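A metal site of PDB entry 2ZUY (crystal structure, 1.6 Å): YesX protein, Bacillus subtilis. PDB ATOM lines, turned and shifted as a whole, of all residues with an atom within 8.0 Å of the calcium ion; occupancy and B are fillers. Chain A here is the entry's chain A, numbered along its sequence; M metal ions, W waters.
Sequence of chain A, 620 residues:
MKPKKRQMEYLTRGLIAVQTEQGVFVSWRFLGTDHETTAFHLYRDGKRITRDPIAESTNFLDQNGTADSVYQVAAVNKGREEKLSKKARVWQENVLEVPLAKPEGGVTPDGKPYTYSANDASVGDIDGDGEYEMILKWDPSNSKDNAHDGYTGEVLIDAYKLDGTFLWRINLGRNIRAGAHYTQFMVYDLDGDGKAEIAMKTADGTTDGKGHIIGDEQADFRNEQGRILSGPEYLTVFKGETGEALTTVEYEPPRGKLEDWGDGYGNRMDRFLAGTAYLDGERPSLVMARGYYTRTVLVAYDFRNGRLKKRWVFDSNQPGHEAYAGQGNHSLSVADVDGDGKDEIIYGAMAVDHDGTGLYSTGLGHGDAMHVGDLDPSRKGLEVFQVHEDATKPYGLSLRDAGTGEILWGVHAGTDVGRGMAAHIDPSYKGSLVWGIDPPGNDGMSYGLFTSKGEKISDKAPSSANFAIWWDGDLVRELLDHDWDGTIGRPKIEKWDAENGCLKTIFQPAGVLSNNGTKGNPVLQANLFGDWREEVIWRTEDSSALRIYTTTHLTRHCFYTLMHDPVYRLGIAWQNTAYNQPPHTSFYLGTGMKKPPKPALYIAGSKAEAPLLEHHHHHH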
ATOM      1  N   TYR A  10       0.613   3.621  14.366  1.00  0.00           N
ATOM      2  CA  TYR A  10       0.769   5.055  14.534  1.00  0.00           C
ATOM      3  C   TYR A  10      -0.496   5.613  15.184  1.00  0.00           C
ATOM      4  O   TYR A  10      -1.602   5.332  14.734  1.00  0.00           O
ATOM      5  CB  TYR A  10       0.983   5.746  13.191  1.00  0.00           C
ATOM      6  CG  TYR A  10       0.989   7.244  13.323  1.00  0.00           C
ATOM      7  CD1 TYR A  10      -0.044   8.016  12.797  1.00  0.00           C
ATOM      8  CD2 TYR A  10       2.026   7.899  13.998  1.00  0.00           C
ATOM      9  CE1 TYR A  10      -0.045   9.393  12.937  1.00  0.00           C
ATOM     10  CE2 TYR A  10       2.028   9.269  14.145  1.00  0.00           C
ATOM     11  CZ  TYR A  10       0.982  10.014  13.610  1.00  0.00           C
ATOM     12  OH  TYR A  10       0.981  11.391  13.751  1.00  0.00           O
ATOM     13  N   GLY A 124      -9.961  -0.221  13.950  1.00  0.00           N
ATOM     14  CA  GLY A 124      -8.713  -0.216  13.221  1.00  0.00           C
ATOM     15  C   GLY A 124      -8.575   1.144  12.576  1.00  0.00           C
ATOM     16  O   GLY A 124      -9.567   1.818  12.326  1.00  0.00           O
ATOM     17  N   ASP A 125      -7.335   1.552  12.337  1.00  0.00           N
ATOM     18  CA  ASP A 125      -7.083   2.786  11.609  1.00  0.00           C
ATOM     19  C   ASP A 125      -7.002   2.416  10.133  1.00  0.00           C
ATOM     20  O   ASP A 125      -5.987   1.913   9.660  1.00  0.00           O
ATOM     21  CB  ASP A 125      -5.788   3.420  12.092  1.00  0.00           C
ATOM     22  CG  ASP A 125      -5.470   4.723  11.377  1.00  0.00           C
ATOM     23  OD1 ASP A 125      -6.310   5.228  10.601  1.00  0.00           O
ATOM     24  OD2 ASP A 125      -4.343   5.231  11.588  1.00  0.00           O
ATOM     25  N   ILE A 126      -8.097   2.629   9.420  1.00  0.00           N
ATOM     26  CA  ILE A 126      -8.197   2.111   8.053  1.00  0.00           C
ATOM     27  C   ILE A 126      -7.505   2.981   7.002  1.00  0.00           C
ATOM     28  O   ILE A 126      -7.243   2.513   5.888  1.00  0.00           O
ATOM     29  CB  ILE A 126      -9.660   1.748   7.660  1.00  0.00           C
ATOM     30  CG1 ILE A 126     -10.634   2.917   7.844  1.00  0.00           C
ATOM     31  CG2 ILE A 126     -10.153   0.593   8.521  1.00  0.00           C
ATOM     32  CD1 ILE A 126     -10.515   4.025   6.824  1.00  0.00           C
ATOM     33  N   ASP A 127      -7.165   4.217   7.376  1.00  0.00           N
ATOM     34  CA  ASP A 127      -6.514   5.155   6.445  1.00  0.00           C
ATOM     35  C   ASP A 127      -5.142   5.673   6.895  1.00  0.00           C
ATOM     36  O   ASP A 127      -4.494   6.441   6.162  1.00  0.00           O
ATOM     37  CB  ASP A 127      -7.460   6.319   6.040  1.00  0.00           C
ATOM     38  CG  ASP A 127      -8.100   7.025   7.225  1.00  0.00           C
ATOM     39  OD1 ASP A 127      -7.784   6.709   8.398  1.00  0.00           O
ATOM     40  OD2 ASP A 127      -8.927   7.924   6.966  1.00  0.00           O
ATOM     41  N   GLY A 128      -4.699   5.244   8.075  1.00  0.00           N
ATOM     42  CA  GLY A 128      -3.335   5.483   8.527  1.00  0.00           C
ATOM     43  C   GLY A 128      -3.043   6.865   9.087  1.00  0.00           C
ATOM     44  O   GLY A 128      -1.889   7.289   9.134  1.00  0.00           O
ATOM     45  N   ASP A 129      -4.086   7.557   9.539  1.00  0.00           N
ATOM     46  CA  ASP A 129      -3.922   8.919  10.049  1.00  0.00           C
ATOM     47  C   ASP A 129      -3.731   9.006  11.577  1.00  0.00           C
ATOM     48  O   ASP A 129      -3.631  10.108  12.129  1.00  0.00           O
ATOM     49  CB  ASP A 129      -5.093   9.799   9.597  1.00  0.00           C
ATOM     50  CG  ASP A 129      -6.385   9.492  10.341  1.00  0.00           C
ATOM     51  OD1 ASP A 129      -7.268  10.368  10.368  1.00  0.00           O
ATOM     52  OD2 ASP A 129      -6.529   8.376  10.881  1.00  0.00           O
ATOM     53  N   GLY A 130      -3.707   7.844  12.232  1.00  0.00           N
ATOM     54  CA  GLY A 130      -3.480   7.788  13.668  1.00  0.00           C
ATOM     55  C   GLY A 130      -4.723   7.928  14.520  1.00  0.00           C
ATOM     56  O   GLY A 130      -4.641   8.142  15.730  1.00  0.00           O
ATOM     57  N   GLU A 131      -5.889   7.794  13.896  1.00  0.00           N
ATOM     58  CA  GLU A 131      -7.172   7.792  14.600  1.00  0.00           C
ATOM     59  C   GLU A 131      -7.957   6.560  14.204  1.00  0.00           C
ATOM     60  O   GLU A 131      -8.009   6.215  13.018  1.00  0.00           O
ATOM     61  CB  GLU A 131      -7.987   9.034  14.263  1.00  0.00           C
ATOM     62  CG  GLU A 131      -7.238  10.366  14.418  1.00  0.00           C
ATOM     63  CD  GLU A 131      -6.989  10.795  15.858  1.00  0.00           C
ATOM     64  OE1 GLU A 131      -6.515  11.911  16.094  1.00  0.00           O
ATOM     65  OE2 GLU A 131      -7.290   9.927  16.820  1.00  0.00           O
ATOM     66  N   TYR A 132      -8.587   5.903  15.176  1.00  0.00           N
ATOM     67  CA  TYR A 132      -9.349   4.693  14.910  1.00  0.00           C
ATOM     68  C   TYR A 132     -10.682   4.961  14.233  1.00  0.00           C
ATOM     69  O   TYR A 132     -11.354   5.935  14.541  1.00  0.00           O
ATOM     70  CB  TYR A 132      -9.619   3.914  16.212  1.00  0.00           C
ATOM     71  CG  TYR A 132      -8.379   3.324  16.822  1.00  0.00           C
ATOM     72  CD1 TYR A 132      -7.669   2.300  16.164  1.00  0.00           C
ATOM     73  CD2 TYR A 132      -7.904   3.771  18.053  1.00  0.00           C
ATOM     74  CE1 TYR A 132      -6.520   1.770  16.715  1.00  0.00           C
ATOM     75  CE2 TYR A 132      -6.758   3.236  18.616  1.00  0.00           C
ATOM     76  CZ  TYR A 132      -6.072   2.228  17.942  1.00  0.00           C
ATOM     77  OH  TYR A 132      -4.939   1.701  18.488  1.00  0.00           O
ATOM     78  N   GLU A 133     -11.023   4.072  13.293  1.00  0.00           N
ATOM     79  CA  GLU A 133     -12.384   3.941  12.769  1.00  0.00           C
ATOM     80  C   GLU A 133     -13.078   2.792  13.503  1.00  0.00           C
ATOM     81  O   GLU A 133     -12.405   1.892  14.050  1.00  0.00           O
ATOM     82  CB  GLU A 133     -12.377   3.638  11.266  1.00  0.00           C
ATOM     83  CG  GLU A 133     -12.095   4.838  10.364  1.00  0.00           C
ATOM     84  CD  GLU A 133     -10.713   5.434  10.568  1.00  0.00           C
ATOM     85  OE1 GLU A 133     -10.628   6.641  10.887  1.00  0.00           O
ATOM     86  OE2 GLU A 133      -9.706   4.716  10.425  1.00  0.00           O
ATOM     87  N   MET A 134     -14.407   2.832  13.516  1.00  0.00           N
ATOM     88  CA  MET A 134     -15.243   1.794  14.117  1.00  0.00           C
ATOM     89  C   MET A 134     -15.666   0.778  13.055  1.00  0.00           C
ATOM     90  O   MET A 134     -16.199   1.169  12.014  1.00  0.00           O
ATOM     91  CB  MET A 134     -16.512   2.406  14.717  1.00  0.00           C
ATOM     92  CG  MET A 134     -16.280   3.455  15.813  1.00  0.00           C
ATOM     93  SD  MET A 134     -15.387   2.840  17.242  1.00  0.00           S
ATOM     94  CE  MET A 134     -16.161   1.237  17.476  1.00  0.00           C
ATOM     95  N   TYR A 160     -17.254   3.136  10.137  1.00  0.00           N
ATOM     96  CA  TYR A 160     -17.575   4.528  10.447  1.00  0.00           C
ATOM     97  C   TYR A 160     -16.368   5.287  10.965  1.00  0.00           C
ATOM     98  O   TYR A 160     -15.566   4.736  11.724  1.00  0.00           O
ATOM     99  CB  TYR A 160     -18.637   4.611  11.542  1.00  0.00           C
ATOM    100  CG  TYR A 160     -19.984   4.078  11.126  1.00  0.00           C
ATOM    101  CD1 TYR A 160     -20.328   2.753  11.381  1.00  0.00           C
ATOM    102  CD2 TYR A 160     -20.906   4.901  10.481  1.00  0.00           C
ATOM    103  CE1 TYR A 160     -21.560   2.247  10.999  1.00  0.00           C
ATOM    104  CE2 TYR A 160     -22.150   4.405  10.099  1.00  0.00           C
ATOM    105  CZ  TYR A 160     -22.458   3.067  10.351  1.00  0.00           C
ATOM    106  OH  TYR A 160     -23.674   2.559   9.974  1.00  0.00           O
ATOM    107  N   LYS A 161     -16.263   6.560  10.585  1.00  0.00           N
ATOM    108  CA  LYS A 161     -15.317   7.464  11.228  1.00  0.00           C
ATOM    109  C   LYS A 161     -15.967   8.020  12.489  1.00  0.00           C
ATOM    110  O   LYS A 161     -17.207   8.040  12.611  1.00  0.00           O
ATOM    111  CB  LYS A 161     -14.886   8.579  10.288  1.00  0.00           C
ATOM    112  CG  LYS A 161     -13.830   8.161   9.293  1.00  0.00           C
ATOM    113  CD  LYS A 161     -13.274   9.344   8.529  1.00  0.00           C
ATOM    114  CE  LYS A 161     -12.041   8.944   7.736  1.00  0.00           C
ATOM    115  NZ  LYS A 161     -10.850   8.773   8.612  1.00  0.00           N
ATOM    116  N   LEU A 162     -15.138   8.465  13.431  1.00  0.00           N
ATOM    117  CA  LEU A 162     -15.614   8.988  14.700  1.00  0.00           C
ATOM    118  C   LEU A 162     -16.487  10.240  14.543  1.00  0.00           C
ATOM    119  O   LEU A 162     -17.279  10.551  15.439  1.00  0.00           O
ATOM    120  CB  LEU A 162     -14.446   9.244  15.653  1.00  0.00           C
ATOM    121  CG  LEU A 162     -13.745   7.968  16.147  1.00  0.00           C
ATOM    122  CD1 LEU A 162     -12.439   8.303  16.849  1.00  0.00           C
ATOM    123  CD2 LEU A 162     -14.645   7.162  17.063  1.00  0.00           C
ATOM    124  N   LEU A 167     -18.600   4.886   5.949  1.00  0.00           N
ATOM    125  CA  LEU A 167     -17.582   4.601   4.919  1.00  0.00           C
ATOM    126  C   LEU A 167     -18.004   3.527   3.937  1.00  0.00           C
ATOM    127  O   LEU A 167     -17.900   3.708   2.728  1.00  0.00           O
ATOM    128  CB  LEU A 167     -16.221   4.259   5.541  1.00  0.00           C
ATOM    129  CG  LEU A 167     -15.608   5.325   6.454  1.00  0.00           C
ATOM    130  CD1 LEU A 167     -14.317   4.829   7.081  1.00  0.00           C
ATOM    131  CD2 LEU A 167     -15.365   6.628   5.681  1.00  0.00           C
ATOM    132  N   GLY A 194       0.419   0.251   7.571  1.00  0.00           N
ATOM    133  CA  GLY A 194      -0.118   1.345   8.364  1.00  0.00           C
ATOM    134  C   GLY A 194      -1.643   1.483   8.324  1.00  0.00           C
ATOM    135  O   GLY A 194      -2.209   2.382   8.966  1.00  0.00           O
HETATM  136 CA    CA M   1      -8.199   6.736  10.702  1.00  0.00          CA
HETATM  137  O   HOH W   1      -9.347   8.963  10.927  1.00  0.00           O
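Residues that only touch the calcium ion: Lys 161 (3.9 Å). Within 4 Å of the calcium ion: Asp 125, Asp 127, Asp 129, Glu 131, Glu 133 and Lys 161.
The side-chain carboxylate (OE2) of Glu 133 sits close to the backbone NH (N) of Ile 126, 2.8 Å away. The side-chain carboxylate of Asp 127 lies within salt-bridge range of the side-chain amino group of Lys 161 (2.7 Å). The side-chain carboxylate of Asp 125 is in hydrogen-bond range of the backbone NH of Gly 130 (2.8 Å). OD1 of Asp 125 sits close to N of Gly 128 (3.0 Å). The side-chain carboxylate (OE1) of Glu 133 sits close to the side-chain amino group (NZ) of Lys 161 (3.1 Å). The backbone carbonyl oxygen of Gly 124 lies within hydrogen-bond range of the backbone NH of Glu 133 (2.9 Å).
Water W1 lies within hydrogen-bond range of the side-chain carboxylate of Asp 129 (2.6 Å) and the side-chain amino group of Lys 161 (2.8 Å).
The calcium ion is bound by the side-chain carboxylate (OD1) of Asp 127, 2.3 Å away. OD2 of Asp 129 binds the calcium ion. O of Glu 131 binds the calcium ion (2.4 Å). OD1 of Asp 125 binds the calcium ion, 2.4 Å away. The calcium ion is bound by OE1 of Glu 133 (2.4 Å). The calcium ion is bound by water W1 (2.5 Å). The calcium ion is bound by the side-chain carboxylate (OE2) of Glu 133, 2.5 Å away. The calcium ion has seven donor atoms within binding distance.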
